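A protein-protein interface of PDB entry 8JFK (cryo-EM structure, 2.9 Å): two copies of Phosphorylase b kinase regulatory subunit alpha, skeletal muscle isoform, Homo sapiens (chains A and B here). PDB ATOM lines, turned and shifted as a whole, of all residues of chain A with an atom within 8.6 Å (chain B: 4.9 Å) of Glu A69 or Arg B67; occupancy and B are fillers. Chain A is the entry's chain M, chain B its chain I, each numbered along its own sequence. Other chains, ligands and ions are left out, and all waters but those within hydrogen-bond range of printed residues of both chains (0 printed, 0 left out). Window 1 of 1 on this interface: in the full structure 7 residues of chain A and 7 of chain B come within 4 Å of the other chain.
Glu A69 touches just these residues of chain B: Arg B2 (3.1 Å) and Arg B67 (3.3 Å).
Of chain A, only Asp A68 and Glu A69 come within 4 Å of Arg B67.
No residue of chain A comes within 4 Å of Asp B66.
Of the printed residues of chain A, Ser B3 touches Asp A12 (3.7 Å) and Lys A73 (3.9 Å).
Of the printed residues of chain B, Asp A68 touches Arg B67 (3.3 Å) and Asp B68 (2.9 Å).
Printed residues of chain A within 4 Å of Arg B2: Glu A69, Lys A73 and Glu A76.
Printed residues of chain A within 4 Å of Glu B69: Arg A67 (2.9 Å).
Val A9 touches none of the printed residues of chain B.
Ser A3 touches none of the printed residues of chain B.
The nearest residue of chain B that does not touch Glu A69 is Ser B3 (4.1 Å).
The nearest residue of chain A that does not touch Arg B67 is Arg A67 (6.0 Å).
The nearest printed residue of chain B that does not touch Lys A73 is Arg B4 (6.0 Å).
Arg A67 touches Asp B68, and with the chains exchanged Asp A68 touches Arg B67.
Arg A67 touches Glu B69, and with the chains exchanged Glu A69 touches Arg B67.
Asp A68 touches its own counterpart, Asp B68.
Positions printed for both chains: 3, 4, 65, 66, 67, 68, 69, 70, 71 and 72.
Of the 10 pairs that touch across the chains among the printed residues, 5 have their exchanged pair printed and touching as well.
The guanidinium group of Arg A67 lies within salt-bridge range of the side-chain carboxylate of Glu B69 (2.9 Å).
The backbone NH (N) of Asp A68 lies within hydrogen-bond range of the side-chain carboxylate (OD2) of Asp B68, at 2.9 Å.
The side-chain carboxylate (OE1) of Glu A69 is in salt-bridge range of the guanidinium group (NH1) of Arg B67, 3.3 Å away.
NE of Arg B2 is in salt-bridge range of OE1 of Glu A76.
OE1 of Glu A69 lies close to O of Arg B2 (3.1 Å).
Of the 21 printed residues of chain A, 6 touch a printed residue of chain B.
Among the printed residues, Asp or Glu carboxylates within 4 Å of a Lys or Arg side-chain nitrogen of the other chain: Arg A67 with Glu B69 (2.9 Å), Glu A69 with Arg B67 (3.3 Å) and Glu A76 with Arg B2 (3.5 Å).
NE of Arg A4 lies within salt-bridge range of OE2 of Glu A69, at 2.4 Å.
N of Asp A12 sits at hydrogen-bond distance from OH of Tyr A61.
The side-chain amino group (NZ) of Lys A73 is in salt-bridge range of the side-chain carboxylate (OD1) of Asp A12 (3.9 Å).
The backbone carbonyl oxygen (O) of Arg B2 is in hydrogen-bond range of the guanidinium group (NH1) of Arg B67 (3.1 Å).
NE of Arg B4 lies within salt-bridge range of OE2 of Glu B69, 3.4 Å away.
The guanidinium group of Arg B67 lies within salt-bridge range of the side-chain carboxylate of Asp B66 (3.7 Å).
Asp A12 touches Ser B3.
Asp B68 touches Arg A67 (OD2 to C, 3.9 Å).
Asp A68 touches Arg B67.
Lys A73 touches Arg B2 (CE to CG, 3.9 Å).
Ser B3 touches Lys A73.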
ATOM      1  N   SER A   3      -3.180 -18.399 -34.777  1.00  0.00           N
ATOM      2  CA  SER A   3      -3.937 -19.161 -33.798  1.00  0.00           C
ATOM      3  C   SER A   3      -2.989 -19.836 -32.815  1.00  0.00           C
ATOM      4  O   SER A   3      -1.784 -19.944 -33.049  1.00  0.00           O
ATOM      5  CB  SER A   3      -4.818 -20.208 -34.484  1.00  0.00           C
ATOM      6  OG  SER A   3      -4.948 -21.369 -33.681  1.00  0.00           O
ATOM      7  N   ARG A   4      -3.553 -20.285 -31.698  1.00  0.00           N
ATOM      8  CA  ARG A   4      -2.768 -21.005 -30.710  1.00  0.00           C
ATOM      9  C   ARG A   4      -2.260 -22.321 -31.287  1.00  0.00           C
ATOM     10  O   ARG A   4      -2.934 -22.982 -32.081  1.00  0.00           O
ATOM     11  CB  ARG A   4      -3.596 -21.277 -29.456  1.00  0.00           C
ATOM     12  CG  ARG A   4      -4.066 -20.030 -28.737  1.00  0.00           C
ATOM     13  CD  ARG A   4      -3.513 -19.981 -27.325  1.00  0.00           C
ATOM     14  NE  ARG A   4      -4.383 -20.665 -26.376  1.00  0.00           N
ATOM     15  CZ  ARG A   4      -3.972 -21.567 -25.496  1.00  0.00           C
ATOM     16  NH1 ARG A   4      -2.698 -21.912 -25.406  1.00  0.00           N
ATOM     17  NH2 ARG A   4      -4.859 -22.135 -24.686  1.00  0.00           N
ATOM     18  N   SER A   5      -1.050 -22.692 -30.882  1.00  0.00           N
ATOM     19  CA  SER A   5      -0.485 -23.965 -31.298  1.00  0.00           C
ATOM     20  C   SER A   5      -1.284 -25.112 -30.696  1.00  0.00           C
ATOM     21  O   SER A   5      -1.918 -24.973 -29.647  1.00  0.00           O
ATOM     22  CB  SER A   5       0.978 -24.065 -30.871  1.00  0.00           C
ATOM     23  OG  SER A   5       1.093 -24.097 -29.459  1.00  0.00           O
ATOM     24  N   GLY A   8      -0.831 -25.747 -27.059  1.00  0.00           N
ATOM     25  CA  GLY A   8      -1.674 -24.961 -26.174  1.00  0.00           C
ATOM     26  C   GLY A   8      -3.090 -25.495 -26.087  1.00  0.00           C
ATOM     27  O   GLY A   8      -3.708 -25.472 -25.020  1.00  0.00           O
ATOM     28  N   VAL A   9      -3.627 -25.978 -27.210  1.00  0.00           N
ATOM     29  CA  VAL A   9      -4.985 -26.515 -27.215  1.00  0.00           C
ATOM     30  C   VAL A   9      -5.073 -27.764 -26.347  1.00  0.00           C
ATOM     31  O   VAL A   9      -6.005 -27.915 -25.546  1.00  0.00           O
ATOM     32  CB  VAL A   9      -5.443 -26.797 -28.658  1.00  0.00           C
ATOM     33  CG1 VAL A   9      -6.906 -27.208 -28.677  1.00  0.00           C
ATOM     34  CG2 VAL A   9      -5.213 -25.575 -29.534  1.00  0.00           C
ATOM     35  N   ASP A  12      -5.037 -27.201 -22.668  1.00  0.00           N
ATOM     36  CA  ASP A  12      -6.317 -26.797 -22.095  1.00  0.00           C
ATOM     37  C   ASP A  12      -7.053 -27.995 -21.511  1.00  0.00           C
ATOM     38  O   ASP A  12      -7.655 -27.899 -20.435  1.00  0.00           O
ATOM     39  CB  ASP A  12      -7.173 -26.098 -23.149  1.00  0.00           C
ATOM     40  CG  ASP A  12      -6.645 -24.724 -23.508  1.00  0.00           C
ATOM     41  OD1 ASP A  12      -5.539 -24.373 -23.049  1.00  0.00           O
ATOM     42  OD2 ASP A  12      -7.337 -23.994 -24.248  1.00  0.00           O
ATOM     43  N   TYR A  61       2.842 -24.346 -20.259  1.00  0.00           N
ATOM     44  CA  TYR A  61       2.206 -23.177 -20.854  1.00  0.00           C
ATOM     45  C   TYR A  61       3.201 -22.058 -21.118  1.00  0.00           C
ATOM     46  O   TYR A  61       3.021 -21.284 -22.065  1.00  0.00           O
ATOM     47  CB  TYR A  61       1.085 -22.665 -19.952  1.00  0.00           C
ATOM     48  CG  TYR A  61      -0.284 -23.177 -20.324  1.00  0.00           C
ATOM     49  CD1 TYR A  61      -0.848 -22.876 -21.557  1.00  0.00           C
ATOM     50  CD2 TYR A  61      -1.018 -23.954 -19.442  1.00  0.00           C
ATOM     51  CE1 TYR A  61      -2.096 -23.341 -21.899  1.00  0.00           C
ATOM     52  CE2 TYR A  61      -2.267 -24.422 -19.775  1.00  0.00           C
ATOM     53  CZ  TYR A  61      -2.802 -24.111 -21.004  1.00  0.00           C
ATOM     54  OH  TYR A  61      -4.050 -24.577 -21.338  1.00  0.00           O
ATOM     55  N   ARG A  62       4.251 -21.952 -20.297  1.00  0.00           N
ATOM     56  CA  ARG A  62       5.212 -20.868 -20.466  1.00  0.00           C
ATOM     57  C   ARG A  62       6.071 -21.076 -21.708  1.00  0.00           C
ATOM     58  O   ARG A  62       6.676 -20.121 -22.208  1.00  0.00           O
ATOM     59  CB  ARG A  62       6.080 -20.748 -19.211  1.00  0.00           C
ATOM     60  CG  ARG A  62       6.980 -19.523 -19.173  1.00  0.00           C
ATOM     61  CD  ARG A  62       6.163 -18.256 -19.385  1.00  0.00           C
ATOM     62  NE  ARG A  62       5.651 -17.708 -18.134  1.00  0.00           N
ATOM     63  CZ  ARG A  62       4.780 -16.711 -18.050  1.00  0.00           C
ATOM     64  NH1 ARG A  62       4.298 -16.122 -19.130  1.00  0.00           N
ATOM     65  NH2 ARG A  62       4.380 -16.298 -16.851  1.00  0.00           N
ATOM     66  N   ASN A  64       5.177 -21.355 -24.630  1.00  0.00           N
ATOM     67  CA  ASN A  64       4.577 -20.715 -25.795  1.00  0.00           C
ATOM     68  C   ASN A  64       3.913 -19.399 -25.412  1.00  0.00           C
ATOM     69  O   ASN A  64       2.902 -19.010 -26.001  1.00  0.00           O
ATOM     70  CB  ASN A  64       3.571 -21.649 -26.467  1.00  0.00           C
ATOM     71  CG  ASN A  64       4.241 -22.812 -27.168  1.00  0.00           C
ATOM     72  OD1 ASN A  64       5.286 -22.653 -27.798  1.00  0.00           O
ATOM     73  ND2 ASN A  64       3.639 -23.990 -27.064  1.00  0.00           N
ATOM     74  N   ALA A  65       4.473 -18.702 -24.426  1.00  0.00           N
ATOM     75  CA  ALA A  65       3.868 -17.489 -23.882  1.00  0.00           C
ATOM     76  C   ALA A  65       4.092 -16.344 -24.860  1.00  0.00           C
ATOM     77  O   ALA A  65       4.990 -15.518 -24.692  1.00  0.00           O
ATOM     78  CB  ALA A  65       4.439 -17.178 -22.504  1.00  0.00           C
ATOM     79  N   ASP A  66       3.261 -16.295 -25.904  1.00  0.00           N
ATOM     80  CA  ASP A  66       3.313 -15.220 -26.887  1.00  0.00           C
ATOM     81  C   ASP A  66       2.000 -14.453 -26.981  1.00  0.00           C
ATOM     82  O   ASP A  66       1.914 -13.482 -27.742  1.00  0.00           O
ATOM     83  CB  ASP A  66       3.701 -15.769 -28.264  1.00  0.00           C
ATOM     84  CG  ASP A  66       2.528 -16.386 -28.998  1.00  0.00           C
ATOM     85  OD1 ASP A  66       1.779 -17.168 -28.379  1.00  0.00           O
ATOM     86  OD2 ASP A  66       2.359 -16.091 -30.201  1.00  0.00           O
ATOM     87  N   ARG A  67       0.980 -14.857 -26.227  1.00  0.00           N
ATOM     88  CA  ARG A  67      -0.312 -14.191 -26.235  1.00  0.00           C
ATOM     89  C   ARG A  67      -0.668 -13.814 -24.806  1.00  0.00           C
ATOM     90  O   ARG A  67      -0.081 -14.322 -23.848  1.00  0.00           O
ATOM     91  CB  ARG A  67      -1.404 -15.082 -26.835  1.00  0.00           C
ATOM     92  CG  ARG A  67      -1.681 -14.828 -28.299  1.00  0.00           C
ATOM     93  CD  ARG A  67      -2.017 -16.126 -29.012  1.00  0.00           C
ATOM     94  NE  ARG A  67      -1.812 -16.028 -30.451  1.00  0.00           N
ATOM     95  CZ  ARG A  67      -0.856 -16.663 -31.113  1.00  0.00           C
ATOM     96  NH1 ARG A  67      -0.003 -17.464 -30.496  1.00  0.00           N
ATOM     97  NH2 ARG A  67      -0.753 -16.491 -32.428  1.00  0.00           N
ATOM     98  N   ASP A  68      -1.639 -12.909 -24.667  1.00  0.00           N
ATOM     99  CA  ASP A  68      -2.018 -12.449 -23.335  1.00  0.00           C
ATOM    100  C   ASP A  68      -2.597 -13.585 -22.503  1.00  0.00           C
ATOM    101  O   ASP A  68      -2.288 -13.712 -21.312  1.00  0.00           O
ATOM    102  CB  ASP A  68      -3.026 -11.302 -23.426  1.00  0.00           C
ATOM    103  CG  ASP A  68      -4.232 -11.645 -24.279  1.00  0.00           C
ATOM    104  OD1 ASP A  68      -4.259 -12.744 -24.870  1.00  0.00           O
ATOM    105  OD2 ASP A  68      -5.160 -10.811 -24.353  1.00  0.00           O
ATOM    106  N   GLU A  69      -3.444 -14.419 -23.109  1.00  0.00           N
ATOM    107  CA  GLU A  69      -4.177 -15.408 -22.328  1.00  0.00           C
ATOM    108  C   GLU A  69      -3.265 -16.538 -21.871  1.00  0.00           C
ATOM    109  O   GLU A  69      -3.307 -16.948 -20.706  1.00  0.00           O
ATOM    110  CB  GLU A  69      -5.363 -15.953 -23.129  1.00  0.00           C
ATOM    111  CG  GLU A  69      -5.018 -16.754 -24.368  1.00  0.00           C
ATOM    112  CD  GLU A  69      -5.969 -17.915 -24.576  1.00  0.00           C
ATOM    113  OE1 GLU A  69      -7.129 -17.821 -24.122  1.00  0.00           O
ATOM    114  OE2 GLU A  69      -5.561 -18.921 -25.188  1.00  0.00           O
ATOM    115  N   ASP A  70      -2.421 -17.047 -22.769  1.00  0.00           N
ATOM    116  CA  ASP A  70      -1.576 -18.175 -22.399  1.00  0.00           C
ATOM    117  C   ASP A  70      -0.336 -17.708 -21.646  1.00  0.00           C
ATOM    118  O   ASP A  70       0.403 -18.526 -21.088  1.00  0.00           O
ATOM    119  CB  ASP A  70      -1.229 -19.005 -23.637  1.00  0.00           C
ATOM    120  CG  ASP A  70      -0.228 -18.330 -24.538  1.00  0.00           C
ATOM    121  OD1 ASP A  70       0.963 -18.298 -24.184  1.00  0.00           O
ATOM    122  OD2 ASP A  70      -0.631 -17.845 -25.613  1.00  0.00           O
ATOM    123  N   LYS A  71      -0.091 -16.397 -21.622  1.00  0.00           N
ATOM    124  CA  LYS A  71       0.789 -15.838 -20.602  1.00  0.00           C
ATOM    125  C   LYS A  71       0.113 -15.856 -19.239  1.00  0.00           C
ATOM    126  O   LYS A  71       0.756 -16.137 -18.221  1.00  0.00           O
ATOM    127  CB  LYS A  71       1.190 -14.408 -20.964  1.00  0.00           C
ATOM    128  CG  LYS A  71       2.483 -14.275 -21.739  1.00  0.00           C
ATOM    129  CD  LYS A  71       2.716 -12.834 -22.164  1.00  0.00           C
ATOM    130  CE  LYS A  71       3.346 -12.754 -23.542  1.00  0.00           C
ATOM    131  NZ  LYS A  71       3.420 -11.351 -24.034  1.00  0.00           N
ATOM    132  N   ALA A  72      -1.187 -15.554 -19.203  1.00  0.00           N
ATOM    133  CA  ALA A  72      -1.882 -15.394 -17.932  1.00  0.00           C
ATOM    134  C   ALA A  72      -2.139 -16.733 -17.254  1.00  0.00           C
ATOM    135  O   ALA A  72      -1.949 -16.861 -16.040  1.00  0.00           O
ATOM    136  CB  ALA A  72      -3.191 -14.636 -18.146  1.00  0.00           C
ATOM    137  N   LYS A  73      -2.573 -17.743 -18.012  1.00  0.00           N
ATOM    138  CA  LYS A  73      -2.781 -19.056 -17.410  1.00  0.00           C
ATOM    139  C   LYS A  73      -1.453 -19.670 -16.993  1.00  0.00           C
ATOM    140  O   LYS A  73      -1.376 -20.401 -16.000  1.00  0.00           O
ATOM    141  CB  LYS A  73      -3.531 -19.979 -18.372  1.00  0.00           C
ATOM    142  CG  LYS A  73      -3.038 -19.933 -19.792  1.00  0.00           C
ATOM    143  CD  LYS A  73      -3.971 -20.668 -20.735  1.00  0.00           C
ATOM    144  CE  LYS A  73      -5.349 -20.038 -20.764  1.00  0.00           C
ATOM    145  NZ  LYS A  73      -6.287 -20.821 -21.613  1.00  0.00           N
ATOM    146  N   ALA A  74      -0.391 -19.381 -17.747  1.00  0.00           N
ATOM    147  CA  ALA A  74       0.949 -19.737 -17.294  1.00  0.00           C
ATOM    148  C   ALA A  74       1.294 -19.006 -16.005  1.00  0.00           C
ATOM    149  O   ALA A  74       1.872 -19.593 -15.085  1.00  0.00           O
ATOM    150  CB  ALA A  74       1.974 -19.421 -18.380  1.00  0.00           C
ATOM    151  N   TYR A  75       0.942 -17.721 -15.921  1.00  0.00           N
ATOM    152  CA  TYR A  75       1.168 -16.962 -14.697  1.00  0.00           C
ATOM    153  C   TYR A  75       0.352 -17.531 -13.543  1.00  0.00           C
ATOM    154  O   TYR A  75       0.852 -17.663 -12.421  1.00  0.00           O
ATOM    155  CB  TYR A  75       0.827 -15.490 -14.928  1.00  0.00           C
ATOM    156  CG  TYR A  75       0.972 -14.617 -13.703  1.00  0.00           C
ATOM    157  CD1 TYR A  75       2.209 -14.115 -13.330  1.00  0.00           C
ATOM    158  CD2 TYR A  75      -0.127 -14.296 -12.921  1.00  0.00           C
ATOM    159  CE1 TYR A  75       2.344 -13.316 -12.216  1.00  0.00           C
ATOM    160  CE2 TYR A  75       0.001 -13.501 -11.804  1.00  0.00           C
ATOM    161  CZ  TYR A  75       1.237 -13.013 -11.457  1.00  0.00           C
ATOM    162  OH  TYR A  75       1.365 -12.218 -10.342  1.00  0.00           O
ATOM    163  N   GLU A  76      -0.914 -17.870 -13.801  1.00  0.00           N
ATOM    164  CA  GLU A  76      -1.758 -18.435 -12.752  1.00  0.00           C
ATOM    165  C   GLU A  76      -1.173 -19.728 -12.210  1.00  0.00           C
ATOM    166  O   GLU A  76      -1.027 -19.887 -10.994  1.00  0.00           O
ATOM    167  CB  GLU A  76      -3.168 -18.691 -13.281  1.00  0.00           C
ATOM    168  CG  GLU A  76      -3.974 -17.452 -13.576  1.00  0.00           C
ATOM    169  CD  GLU A  76      -5.334 -17.776 -14.157  1.00  0.00           C
ATOM    170  OE1 GLU A  76      -5.455 -17.826 -15.399  1.00  0.00           O
ATOM    171  OE2 GLU A  76      -6.281 -17.992 -13.373  1.00  0.00           O
ATOM    172  N   ARG B   2     -11.849 -17.643 -19.917  1.00  0.00           N
ATOM    173  CA  ARG B   2     -10.430 -17.977 -19.997  1.00  0.00           C
ATOM    174  C   ARG B   2     -10.061 -18.438 -21.400  1.00  0.00           C
ATOM    175  O   ARG B   2      -9.497 -17.674 -22.184  1.00  0.00           O
ATOM    176  CB  ARG B   2     -10.074 -19.052 -18.974  1.00  0.00           C
ATOM    177  CG  ARG B   2      -8.584 -19.244 -18.770  1.00  0.00           C
ATOM    178  CD  ARG B   2      -8.220 -20.124 -17.564  1.00  0.00           C
ATOM    179  NE  ARG B   2      -8.392 -19.473 -16.266  1.00  0.00           N
ATOM    180  CZ  ARG B   2      -9.545 -19.273 -15.640  1.00  0.00           C
ATOM    181  NH1 ARG B   2     -10.681 -19.776 -16.096  1.00  0.00           N
ATOM    182  NH2 ARG B   2      -9.553 -18.582 -14.504  1.00  0.00           N
ATOM    183  N   SER B   3     -10.376 -19.688 -21.711  1.00  0.00           N
ATOM    184  CA  SER B   3     -10.221 -20.212 -23.057  1.00  0.00           C
ATOM    185  C   SER B   3     -11.198 -19.506 -23.989  1.00  0.00           C
ATOM    186  O   SER B   3     -12.280 -19.076 -23.581  1.00  0.00           O
ATOM    187  CB  SER B   3     -10.458 -21.724 -23.089  1.00  0.00           C
ATOM    188  OG  SER B   3      -9.804 -22.366 -22.008  1.00  0.00           O
ATOM    189  N   ARG B   4     -10.796 -19.381 -25.249  1.00  0.00           N
ATOM    190  CA  ARG B   4     -11.618 -18.672 -26.217  1.00  0.00           C
ATOM    191  C   ARG B   4     -12.955 -19.374 -26.412  1.00  0.00           C
ATOM    192  O   ARG B   4     -13.068 -20.596 -26.294  1.00  0.00           O
ATOM    193  CB  ARG B   4     -10.896 -18.555 -27.557  1.00  0.00           C
ATOM    194  CG  ARG B   4      -9.612 -17.758 -27.506  1.00  0.00           C
ATOM    195  CD  ARG B   4      -9.357 -17.095 -28.844  1.00  0.00           C
ATOM    196  NE  ARG B   4      -9.625 -18.004 -29.951  1.00  0.00           N
ATOM    197  CZ  ARG B   4      -9.844 -17.620 -31.200  1.00  0.00           C
ATOM    198  NH1 ARG B   4      -9.826 -16.343 -31.545  1.00  0.00           N
ATOM    199  NH2 ARG B   4     -10.086 -18.540 -32.130  1.00  0.00           N
ATOM    200  N   ALA B  65     -14.342  -9.997 -29.580  1.00  0.00           N
ATOM    201  CA  ALA B  65     -12.927  -9.627 -29.559  1.00  0.00           C
ATOM    202  C   ALA B  65     -12.583  -9.062 -28.188  1.00  0.00           C
ATOM    203  O   ALA B  65     -12.471  -7.850 -27.999  1.00  0.00           O
ATOM    204  CB  ALA B  65     -12.616  -8.631 -30.670  1.00  0.00           C
ATOM    205  N   ASP B  66     -12.412  -9.956 -27.216  1.00  0.00           N
ATOM    206  CA  ASP B  66     -11.976  -9.581 -25.877  1.00  0.00           C
ATOM    207  C   ASP B  66     -10.518  -9.940 -25.627  1.00  0.00           C
ATOM    208  O   ASP B  66     -10.033  -9.786 -24.500  1.00  0.00           O
ATOM    209  CB  ASP B  66     -12.869 -10.244 -24.824  1.00  0.00           C
ATOM    210  CG  ASP B  66     -12.411 -11.644 -24.466  1.00  0.00           C
ATOM    211  OD1 ASP B  66     -12.630 -12.568 -25.277  1.00  0.00           O
ATOM    212  OD2 ASP B  66     -11.833 -11.820 -23.373  1.00  0.00           O
ATOM    213  N   ARG B  67      -9.807 -10.400 -26.652  1.00  0.00           N
ATOM    214  CA  ARG B  67      -8.456 -10.916 -26.510  1.00  0.00           C
ATOM    215  C   ARG B  67      -7.617 -10.368 -27.656  1.00  0.00           C
ATOM    216  O   ARG B  67      -8.139 -10.057 -28.727  1.00  0.00           O
ATOM    217  CB  ARG B  67      -8.479 -12.450 -26.494  1.00  0.00           C
ATOM    218  CG  ARG B  67      -7.138 -13.140 -26.512  1.00  0.00           C
ATOM    219  CD  ARG B  67      -7.266 -14.492 -25.843  1.00  0.00           C
ATOM    220  NE  ARG B  67      -8.662 -14.846 -25.608  1.00  0.00           N
ATOM    221  CZ  ARG B  67      -9.191 -15.068 -24.411  1.00  0.00           C
ATOM    222  NH1 ARG B  67      -8.474 -14.957 -23.308  1.00  0.00           N
ATOM    223  NH2 ARG B  67     -10.475 -15.403 -24.322  1.00  0.00           N
ATOM    224  N   ASP B  68      -6.305 -10.255 -27.422  1.00  0.00           N
ATOM    225  CA  ASP B  68      -5.452  -9.527 -28.360  1.00  0.00           C
ATOM    226  C   ASP B  68      -5.514 -10.129 -29.757  1.00  0.00           C
ATOM    227  O   ASP B  68      -5.626  -9.399 -30.748  1.00  0.00           O
ATOM    228  CB  ASP B  68      -4.004  -9.501 -27.871  1.00  0.00           C
ATOM    229  CG  ASP B  68      -3.552 -10.830 -27.306  1.00  0.00           C
ATOM    230  OD1 ASP B  68      -4.187 -11.860 -27.612  1.00  0.00           O
ATOM    231  OD2 ASP B  68      -2.539 -10.847 -26.575  1.00  0.00           O
ATOM    232  N   GLU B  69      -5.434 -11.457 -29.863  1.00  0.00           N
ATOM    233  CA  GLU B  69      -5.479 -12.078 -31.183  1.00  0.00           C
ATOM    234  C   GLU B  69      -6.847 -11.894 -31.824  1.00  0.00           C
ATOM    235  O   GLU B  69      -6.946 -11.601 -33.019  1.00  0.00           O
ATOM    236  CB  GLU B  69      -5.098 -13.557 -31.100  1.00  0.00           C
ATOM    237  CG  GLU B  69      -5.987 -14.428 -30.239  1.00  0.00           C
ATOM    238  CD  GLU B  69      -5.680 -15.900 -30.427  1.00  0.00           C
ATOM    239  OE1 GLU B  69      -4.620 -16.215 -31.008  1.00  0.00           O
ATOM    240  OE2 GLU B  69      -6.491 -16.743 -29.997  1.00  0.00           O
ATOM    241  N   ASP B  70      -7.917 -12.035 -31.034  1.00  0.00           N
ATOM    242  CA  ASP B  70      -9.261 -11.817 -31.560  1.00  0.00           C
ATOM    243  C   ASP B  70      -9.443 -10.381 -32.032  1.00  0.00           C
ATOM    244  O   ASP B  70     -10.081 -10.136 -33.060  1.00  0.00           O
ATOM    245  CB  ASP B  70     -10.305 -12.165 -30.500  1.00  0.00           C
ATOM    246  CG  ASP B  70     -10.843 -13.571 -30.654  1.00  0.00           C
ATOM    247  OD1 ASP B  70     -10.784 -14.110 -31.779  1.00  0.00           O
ATOM    248  OD2 ASP B  70     -11.326 -14.139 -29.652  1.00  0.00           O
ATOM    249  N   LYS B  71      -8.896  -9.420 -31.286  1.00  0.00           N
ATOM    250  CA  LYS B  71      -8.875  -8.044 -31.766  1.00  0.00           C
ATOM    251  C   LYS B  71      -8.060  -7.926 -33.046  1.00  0.00           C
ATOM    252  O   LYS B  71      -8.448  -7.205 -33.971  1.00  0.00           O
ATOM    253  CB  LYS B  71      -8.307  -7.118 -30.690  1.00  0.00           C
ATOM    254  CG  LYS B  71      -9.055  -7.134 -29.374  1.00  0.00           C
ATOM    255  CD  LYS B  71      -8.939  -5.798 -28.667  1.00  0.00           C
ATOM    256  CE  LYS B  71      -9.030  -5.960 -27.163  1.00  0.00           C
ATOM    257  NZ  LYS B  71      -8.271  -4.901 -26.444  1.00  0.00           N
ATOM    258  N   ALA B  72      -6.932  -8.634 -33.119  1.00  0.00           N
ATOM    259  CA  ALA B  72      -6.020  -8.463 -34.244  1.00  0.00           C
ATOM    260  C   ALA B  72      -6.560  -9.109 -35.514  1.00  0.00           C
ATOM    261  O   ALA B  72      -6.421  -8.547 -36.606  1.00  0.00           O
ATOM    262  CB  ALA B  72      -4.645  -9.029 -33.892  1.00  0.00           C
